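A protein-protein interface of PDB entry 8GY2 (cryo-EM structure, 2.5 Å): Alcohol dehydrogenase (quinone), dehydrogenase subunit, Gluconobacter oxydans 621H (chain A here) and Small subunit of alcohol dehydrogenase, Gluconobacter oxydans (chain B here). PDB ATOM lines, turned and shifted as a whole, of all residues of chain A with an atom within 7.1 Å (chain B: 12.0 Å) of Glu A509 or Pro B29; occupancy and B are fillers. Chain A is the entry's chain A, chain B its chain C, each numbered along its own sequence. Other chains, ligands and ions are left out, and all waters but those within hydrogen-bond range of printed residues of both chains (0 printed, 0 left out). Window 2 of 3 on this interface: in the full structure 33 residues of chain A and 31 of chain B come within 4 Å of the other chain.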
ATOM      1  N   MET A 354       1.459 -25.441  25.739  1.00  0.00           N
ATOM      2  CA  MET A 354       0.168 -25.127  25.150  1.00  0.00           C
ATOM      3  C   MET A 354       0.215 -25.306  23.643  1.00  0.00           C
ATOM      4  O   MET A 354       1.266 -25.129  23.025  1.00  0.00           O
ATOM      5  CB  MET A 354      -0.246 -23.685  25.474  1.00  0.00           C
ATOM      6  CG  MET A 354      -0.519 -23.433  26.941  1.00  0.00           C
ATOM      7  SD  MET A 354      -1.173 -21.783  27.240  1.00  0.00           S
ATOM      8  CE  MET A 354      -1.806 -21.365  25.620  1.00  0.00           C
ATOM      9  N   PRO A 355      -0.909 -25.657  23.025  1.00  0.00           N
ATOM     10  CA  PRO A 355      -0.955 -25.734  21.549  1.00  0.00           C
ATOM     11  C   PRO A 355      -1.114 -24.362  20.898  1.00  0.00           C
ATOM     12  O   PRO A 355      -2.196 -23.919  20.517  1.00  0.00           O
ATOM     13  CB  PRO A 355      -2.163 -26.637  21.297  1.00  0.00           C
ATOM     14  CG  PRO A 355      -3.045 -26.417  22.473  1.00  0.00           C
ATOM     15  CD  PRO A 355      -2.140 -26.175  23.646  1.00  0.00           C
ATOM     16  N   VAL A 356       0.005 -23.656  20.768  1.00  0.00           N
ATOM     17  CA  VAL A 356       0.012 -22.344  20.129  1.00  0.00           C
ATOM     18  C   VAL A 356       0.075 -22.530  18.620  1.00  0.00           C
ATOM     19  O   VAL A 356       0.962 -23.221  18.104  1.00  0.00           O
ATOM     20  CB  VAL A 356       1.190 -21.498  20.636  1.00  0.00           C
ATOM     21  CG1 VAL A 356       1.229 -20.161  19.915  1.00  0.00           C
ATOM     22  CG2 VAL A 356       1.090 -21.294  22.137  1.00  0.00           C
ATOM     23  N   ASN A 357      -0.868 -21.909  17.909  1.00  0.00           N
ATOM     24  CA  ASN A 357      -0.976 -22.024  16.453  1.00  0.00           C
ATOM     25  C   ASN A 357      -1.084 -23.484  16.019  1.00  0.00           C
ATOM     26  O   ASN A 357      -0.495 -23.899  15.018  1.00  0.00           O
ATOM     27  CB  ASN A 357       0.196 -21.332  15.752  1.00  0.00           C
ATOM     28  CG  ASN A 357       0.207 -19.832  15.974  1.00  0.00           C
ATOM     29  OD1 ASN A 357      -0.820 -19.232  16.282  1.00  0.00           O
ATOM     30  ND2 ASN A 357       1.375 -19.221  15.820  1.00  0.00           N
ATOM     31  N   GLY A 358      -1.846 -24.267  16.776  1.00  0.00           N
ATOM     32  CA  GLY A 358      -1.998 -25.681  16.473  1.00  0.00           C
ATOM     33  C   GLY A 358      -0.720 -26.476  16.603  1.00  0.00           C
ATOM     34  O   GLY A 358      -0.540 -27.471  15.896  1.00  0.00           O
ATOM     35  N   ILE A 375       0.750 -14.348  27.887  1.00  0.00           N
ATOM     36  CA  ILE A 375       1.376 -15.580  27.426  1.00  0.00           C
ATOM     37  C   ILE A 375       2.511 -15.178  26.500  1.00  0.00           C
ATOM     38  O   ILE A 375       2.284 -14.487  25.497  1.00  0.00           O
ATOM     39  CB  ILE A 375       0.382 -16.502  26.703  1.00  0.00           C
ATOM     40  CG1 ILE A 375      -0.765 -16.895  27.634  1.00  0.00           C
ATOM     41  CG2 ILE A 375       1.092 -17.735  26.171  1.00  0.00           C
ATOM     42  CD1 ILE A 375      -1.791 -17.785  26.977  1.00  0.00           C
ATOM     43  N   ILE A 384       3.373 -13.462  22.798  1.00  0.00           N
ATOM     44  CA  ILE A 384       2.392 -14.271  22.084  1.00  0.00           C
ATOM     45  C   ILE A 384       1.023 -13.609  22.179  1.00  0.00           C
ATOM     46  O   ILE A 384       0.417 -13.270  21.156  1.00  0.00           O
ATOM     47  CB  ILE A 384       2.346 -15.713  22.621  1.00  0.00           C
ATOM     48  CG1 ILE A 384       3.666 -16.430  22.333  1.00  0.00           C
ATOM     49  CG2 ILE A 384       1.182 -16.472  22.008  1.00  0.00           C
ATOM     50  CD1 ILE A 384       3.784 -17.778  23.003  1.00  0.00           C
ATOM     51  N   THR A 385       0.527 -13.417  23.398  1.00  0.00           N
ATOM     52  CA  THR A 385      -0.783 -12.802  23.566  1.00  0.00           C
ATOM     53  C   THR A 385      -0.889 -12.184  24.953  1.00  0.00           C
ATOM     54  O   THR A 385      -0.105 -12.489  25.854  1.00  0.00           O
ATOM     55  CB  THR A 385      -1.915 -13.813  23.345  1.00  0.00           C
ATOM     56  OG1 THR A 385      -3.143 -13.115  23.115  1.00  0.00           O
ATOM     57  CG2 THR A 385      -2.071 -14.716  24.555  1.00  0.00           C
ATOM     58  N   GLY A 386      -1.874 -11.304  25.105  1.00  0.00           N
ATOM     59  CA  GLY A 386      -2.149 -10.679  26.382  1.00  0.00           C
ATOM     60  C   GLY A 386      -3.518 -10.036  26.426  1.00  0.00           C
ATOM     61  O   GLY A 386      -3.880  -9.271  25.528  1.00  0.00           O
ATOM     62  N   LYS A 387      -4.289 -10.335  27.467  1.00  0.00           N
ATOM     63  CA  LYS A 387      -5.645  -9.809  27.575  1.00  0.00           C
ATOM     64  C   LYS A 387      -5.965  -9.542  29.035  1.00  0.00           C
ATOM     65  O   LYS A 387      -5.475 -10.259  29.910  1.00  0.00           O
ATOM     66  CB  LYS A 387      -6.678 -10.780  26.982  1.00  0.00           C
ATOM     67  CG  LYS A 387      -6.857 -10.658  25.479  1.00  0.00           C
ATOM     68  CD  LYS A 387      -7.871 -11.664  24.964  1.00  0.00           C
ATOM     69  CE  LYS A 387      -7.900 -11.689  23.447  1.00  0.00           C
ATOM     70  NZ  LYS A 387      -9.273 -11.464  22.917  1.00  0.00           N
ATOM     71  N   LYS A 442      -6.778 -28.008  32.481  1.00  0.00           N
ATOM     72  CA  LYS A 442      -6.032 -27.027  31.691  1.00  0.00           C
ATOM     73  C   LYS A 442      -6.403 -25.601  32.085  1.00  0.00           C
ATOM     74  O   LYS A 442      -6.559 -24.724  31.233  1.00  0.00           O
ATOM     75  CB  LYS A 442      -6.244 -27.244  30.190  1.00  0.00           C
ATOM     76  CG  LYS A 442      -6.139 -28.688  29.739  1.00  0.00           C
ATOM     77  CD  LYS A 442      -4.693 -29.113  29.572  1.00  0.00           C
ATOM     78  CE  LYS A 442      -4.519 -29.998  28.349  1.00  0.00           C
ATOM     79  NZ  LYS A 442      -5.812 -30.575  27.891  1.00  0.00           N
ATOM     80  N   TRP A 506      -8.937 -18.922  34.775  1.00  0.00           N
ATOM     81  CA  TRP A 506      -8.576 -18.503  33.431  1.00  0.00           C
ATOM     82  C   TRP A 506      -8.288 -19.710  32.548  1.00  0.00           C
ATOM     83  O   TRP A 506      -7.690 -20.698  32.988  1.00  0.00           O
ATOM     84  CB  TRP A 506      -7.354 -17.587  33.483  1.00  0.00           C
ATOM     85  CG  TRP A 506      -7.173 -16.729  32.275  1.00  0.00           C
ATOM     86  CD1 TRP A 506      -6.235 -16.878  31.297  1.00  0.00           C
ATOM     87  CD2 TRP A 506      -7.945 -15.578  31.918  1.00  0.00           C
ATOM     88  NE1 TRP A 506      -6.377 -15.894  30.352  1.00  0.00           N
ATOM     89  CE2 TRP A 506      -7.420 -15.083  30.710  1.00  0.00           C
ATOM     90  CE3 TRP A 506      -9.031 -14.920  32.501  1.00  0.00           C
ATOM     91  CZ2 TRP A 506      -7.943 -13.959  30.074  1.00  0.00           C
ATOM     92  CZ3 TRP A 506      -9.549 -13.808  31.868  1.00  0.00           C
ATOM     93  CH2 TRP A 506      -9.005 -13.338  30.668  1.00  0.00           C
ATOM     94  N   ASP A 507      -8.717 -19.621  31.291  1.00  0.00           N
ATOM     95  CA  ASP A 507      -8.429 -20.636  30.284  1.00  0.00           C
ATOM     96  C   ASP A 507      -7.451 -20.046  29.278  1.00  0.00           C
ATOM     97  O   ASP A 507      -7.859 -19.272  28.400  1.00  0.00           O
ATOM     98  CB  ASP A 507      -9.714 -21.089  29.583  1.00  0.00           C
ATOM     99  CG  ASP A 507      -9.540 -22.389  28.823  1.00  0.00           C
ATOM    100  OD1 ASP A 507      -8.384 -22.810  28.611  1.00  0.00           O
ATOM    101  OD2 ASP A 507     -10.562 -22.989  28.433  1.00  0.00           O
ATOM    102  N   PRO A 508      -6.158 -20.367  29.367  1.00  0.00           N
ATOM    103  CA  PRO A 508      -5.183 -19.738  28.464  1.00  0.00           C
ATOM    104  C   PRO A 508      -5.437 -20.013  26.992  1.00  0.00           C
ATOM    105  O   PRO A 508      -5.133 -19.158  26.153  1.00  0.00           O
ATOM    106  CB  PRO A 508      -3.845 -20.331  28.928  1.00  0.00           C
ATOM    107  CG  PRO A 508      -4.095 -20.813  30.318  1.00  0.00           C
ATOM    108  CD  PRO A 508      -5.516 -21.271  30.334  1.00  0.00           C
ATOM    109  N   GLU A 509      -5.978 -21.185  26.650  1.00  0.00           N
ATOM    110  CA  GLU A 509      -6.254 -21.489  25.250  1.00  0.00           C
ATOM    111  C   GLU A 509      -7.295 -20.540  24.671  1.00  0.00           C
ATOM    112  O   GLU A 509      -7.163 -20.083  23.530  1.00  0.00           O
ATOM    113  CB  GLU A 509      -6.712 -22.940  25.108  1.00  0.00           C
ATOM    114  CG  GLU A 509      -5.619 -23.894  24.664  1.00  0.00           C
ATOM    115  CD  GLU A 509      -5.406 -23.875  23.164  1.00  0.00           C
ATOM    116  OE1 GLU A 509      -6.147 -24.583  22.448  1.00  0.00           O
ATOM    117  OE2 GLU A 509      -4.498 -23.157  22.698  1.00  0.00           O
ATOM    118  N   LYS A 510      -8.338 -20.236  25.438  1.00  0.00           N
ATOM    119  CA  LYS A 510      -9.370 -19.304  25.005  1.00  0.00           C
ATOM    120  C   LYS A 510      -9.121 -17.879  25.478  1.00  0.00           C
ATOM    121  O   LYS A 510      -9.755 -16.955  24.957  1.00  0.00           O
ATOM    122  CB  LYS A 510     -10.742 -19.767  25.505  1.00  0.00           C
ATOM    123  CG  LYS A 510     -11.095 -21.193  25.127  1.00  0.00           C
ATOM    124  CD  LYS A 510     -12.497 -21.548  25.591  1.00  0.00           C
ATOM    125  CE  LYS A 510     -13.042 -22.753  24.843  1.00  0.00           C
ATOM    126  NZ  LYS A 510     -11.998 -23.411  24.010  1.00  0.00           N
ATOM    127  N   MET A 511      -8.216 -17.688  26.438  1.00  0.00           N
ATOM    128  CA  MET A 511      -7.961 -16.381  27.047  1.00  0.00           C
ATOM    129  C   MET A 511      -9.254 -15.767  27.574  1.00  0.00           C
ATOM    130  O   MET A 511      -9.509 -14.570  27.427  1.00  0.00           O
ATOM    131  CB  MET A 511      -7.256 -15.440  26.069  1.00  0.00           C
ATOM    132  CG  MET A 511      -5.856 -15.895  25.698  1.00  0.00           C
ATOM    133  SD  MET A 511      -4.634 -15.589  26.988  1.00  0.00           S
ATOM    134  CE  MET A 511      -4.834 -13.833  27.253  1.00  0.00           C
ATOM    135  N   ALA A 512     -10.081 -16.605  28.191  1.00  0.00           N
ATOM    136  CA  ALA A 512     -11.350 -16.206  28.772  1.00  0.00           C
ATOM    137  C   ALA A 512     -11.527 -16.922  30.102  1.00  0.00           C
ATOM    138  O   ALA A 512     -10.982 -18.015  30.296  1.00  0.00           O
ATOM    139  CB  ALA A 512     -12.527 -16.540  27.841  1.00  0.00           C
ATOM    140  N   GLU B  26      -4.130 -17.009  12.985  1.00  0.00           N
ATOM    141  CA  GLU B  26      -3.921 -17.270  14.403  1.00  0.00           C
ATOM    142  C   GLU B  26      -4.760 -18.450  14.884  1.00  0.00           C
ATOM    143  O   GLU B  26      -4.354 -19.605  14.750  1.00  0.00           O
ATOM    144  CB  GLU B  26      -4.249 -16.026  15.232  1.00  0.00           C
ATOM    145  CG  GLU B  26      -3.532 -15.961  16.573  1.00  0.00           C
ATOM    146  CD  GLU B  26      -2.257 -15.142  16.521  1.00  0.00           C
ATOM    147  OE1 GLU B  26      -2.083 -14.369  15.555  1.00  0.00           O
ATOM    148  OE2 GLU B  26      -1.431 -15.267  17.449  1.00  0.00           O
ATOM    149  N   GLN B  27      -5.926 -18.146  15.454  1.00  0.00           N
ATOM    150  CA  GLN B  27      -6.837 -19.110  16.069  1.00  0.00           C
ATOM    151  C   GLN B  27      -6.186 -19.880  17.213  1.00  0.00           C
ATOM    152  O   GLN B  27      -6.768 -20.845  17.723  1.00  0.00           O
ATOM    153  CB  GLN B  27      -7.420 -20.077  15.030  1.00  0.00           C
ATOM    154  CG  GLN B  27      -7.820 -19.391  13.730  1.00  0.00           C
ATOM    155  CD  GLN B  27      -9.321 -19.325  13.538  1.00  0.00           C
ATOM    156  OE1 GLN B  27     -10.079 -19.999  14.234  1.00  0.00           O
ATOM    157  NE2 GLN B  27      -9.760 -18.500  12.595  1.00  0.00           N
ATOM    158  N   SER B  28      -4.994 -19.465  17.624  1.00  0.00           N
ATOM    159  CA  SER B  28      -4.285 -19.825  18.842  1.00  0.00           C
ATOM    160  C   SER B  28      -4.948 -19.053  19.977  1.00  0.00           C
ATOM    161  O   SER B  28      -6.001 -18.445  19.747  1.00  0.00           O
ATOM    162  CB  SER B  28      -2.800 -19.484  18.703  1.00  0.00           C
ATOM    163  OG  SER B  28      -2.507 -18.222  19.277  1.00  0.00           O
ATOM    164  N   PRO B  29      -4.439 -19.103  21.210  1.00  0.00           N
ATOM    165  CA  PRO B  29      -4.858 -18.118  22.205  1.00  0.00           C
ATOM    166  C   PRO B  29      -4.960 -16.745  21.568  1.00  0.00           C
ATOM    167  O   PRO B  29      -3.961 -16.213  21.060  1.00  0.00           O
ATOM    168  CB  PRO B  29      -3.734 -18.170  23.253  1.00  0.00           C
ATOM    169  CG  PRO B  29      -2.839 -19.341  22.850  1.00  0.00           C
ATOM    170  CD  PRO B  29      -3.591 -20.132  21.829  1.00  0.00           C
ATOM    171  N   PRO B  30      -6.155 -16.158  21.557  1.00  0.00           N
ATOM    172  CA  PRO B  30      -6.423 -15.067  20.626  1.00  0.00           C
ATOM    173  C   PRO B  30      -5.514 -13.885  20.885  1.00  0.00           C
ATOM    174  O   PRO B  30      -5.178 -13.577  22.045  1.00  0.00           O
ATOM    175  CB  PRO B  30      -7.895 -14.721  20.901  1.00  0.00           C
ATOM    176  CG  PRO B  30      -8.200 -15.316  22.232  1.00  0.00           C
ATOM    177  CD  PRO B  30      -7.341 -16.525  22.346  1.00  0.00           C
ATOM    178  N   PRO B  31      -5.088 -13.193  19.835  1.00  0.00           N
ATOM    179  CA  PRO B  31      -4.241 -12.019  20.010  1.00  0.00           C
ATOM    180  C   PRO B  31      -5.064 -10.835  20.479  1.00  0.00           C
ATOM    181  O   PRO B  31      -6.303 -10.881  20.443  1.00  0.00           O
ATOM    182  CB  PRO B  31      -3.678 -11.786  18.601  1.00  0.00           C
ATOM    183  CG  PRO B  31      -4.756 -12.280  17.701  1.00  0.00           C
ATOM    184  CD  PRO B  31      -5.433 -13.423  18.421  1.00  0.00           C
ATOM    185  N   PRO B  32      -4.423  -9.766  20.942  1.00  0.00           N
ATOM    186  CA  PRO B  32      -5.164  -8.554  21.290  1.00  0.00           C
ATOM    187  C   PRO B  32      -5.922  -8.025  20.088  1.00  0.00           C
ATOM    188  O   PRO B  32      -5.431  -8.100  18.951  1.00  0.00           O
ATOM    189  CB  PRO B  32      -4.062  -7.579  21.730  1.00  0.00           C
ATOM    190  CG  PRO B  32      -2.945  -8.452  22.170  1.00  0.00           C
ATOM    191  CD  PRO B  32      -2.992  -9.655  21.279  1.00  0.00           C
ATOM    192  N   PRO B  33      -7.125  -7.497  20.292  1.00  0.00           N
ATOM    193  CA  PRO B  33      -7.917  -7.010  19.158  1.00  0.00           C
ATOM    194  C   PRO B  33      -7.249  -5.828  18.476  1.00  0.00           C
ATOM    195  O   PRO B  33      -6.491  -5.071  19.089  1.00  0.00           O
ATOM    196  CB  PRO B  33      -9.247  -6.603  19.801  1.00  0.00           C
ATOM    197  CG  PRO B  33      -8.917  -6.351  21.232  1.00  0.00           C
ATOM    198  CD  PRO B  33      -7.817  -7.308  21.577  1.00  0.00           C
ATOM    199  N   ALA B  34      -7.532  -5.687  17.183  1.00  0.00           N
ATOM    200  CA  ALA B  34      -6.952  -4.601  16.406  1.00  0.00           C
ATOM    201  C   ALA B  34      -7.375  -3.251  16.972  1.00  0.00           C
ATOM    202  O   ALA B  34      -8.534  -3.050  17.345  1.00  0.00           O
ATOM    203  CB  ALA B  34      -7.374  -4.714  14.941  1.00  0.00           C
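Of the 18 printed residues of chain A, 9 touch a printed residue of chain B.
Along chain A the printed residues that touch a printed residue of chain B span positions 354 to 511.
Printed residues of chain B that touch a printed residue of chain A: Glu B26, Ser B28, Pro B29, Pro B30, Pro B31 and Pro B32.
Hydrophobic or aromatic side chains of chain B within 4 Å of the printed part of chain A: Pro B29, Pro B30 and Pro B32.
No residue of chain B comes within 4 Å of Pro A355.
Printed residues of chain B within 4 Å of Asn A357: Glu B26 (3.9 Å) and Ser B28 (3.1 Å).
No residue of chain B comes within 4 Å of Ile A375.
Of the printed residues of chain B, Lys A387 touches Pro B30 and Pro B31.
Of chain B, only Pro B29 comes within 4 Å of Pro A508.
Of chain B, only Pro B29 and Pro B30 come within 4 Å of Glu A509.
Of the printed residues of chain B, Met A511 touches Pro B29 (3.96 Å) and Pro B30 (3.7 Å).
Gln B27 touches none of the printed residues of chain A.
Of chain A, only Met A354 (3.6 Å), Thr A385 (3.8 Å), Pro A508 (3.4 Å), Glu A509 (3.3 Å) and Met A511 (3.96 Å) come within 4 Å of Pro B29.
Ala B34 touches none of the printed residues of chain A.
The nearest residue of chain B that does not touch Glu A509 is Ser B28 (4.3 Å).
Among the printed residues, merely in contact across the chains: Met A354 with Pro B29 (3.6 Å), Asn A357 with Glu B26 (3.9 Å), Asn A357 with Ser B28 (3.1 Å), Thr A385 with Pro B29 (3.8 Å), Thr A385 with Pro B31 (3.5 Å), Thr A385 with Pro B32 (3.9 Å), Gly A386 with Pro B32 (3.6 Å), Lys A387 with Pro B30 (3.6 Å), Lys A387 with Pro B31 (3.5 Å), Pro A508 with Pro B29 (3.4 Å), Glu A509 with Pro B29 (3.3 Å), Glu A509 with Pro B30 (3.8 Å), Lys A510 with Pro B30 (3.5 Å), Met A511 with Pro B29 (3.96 Å) and Met A511 with Pro B30 (3.7 Å).
The side-chain hydroxyl (OG1) of Thr A385 lies close to the backbone carbonyl oxygen (O) of Pro B30, 2.3 Å away.
The backbone carbonyl oxygen (O) of Thr A385 is in hydrogen-bond range of the backbone NH (N) of Ile A375 (2.9 Å).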
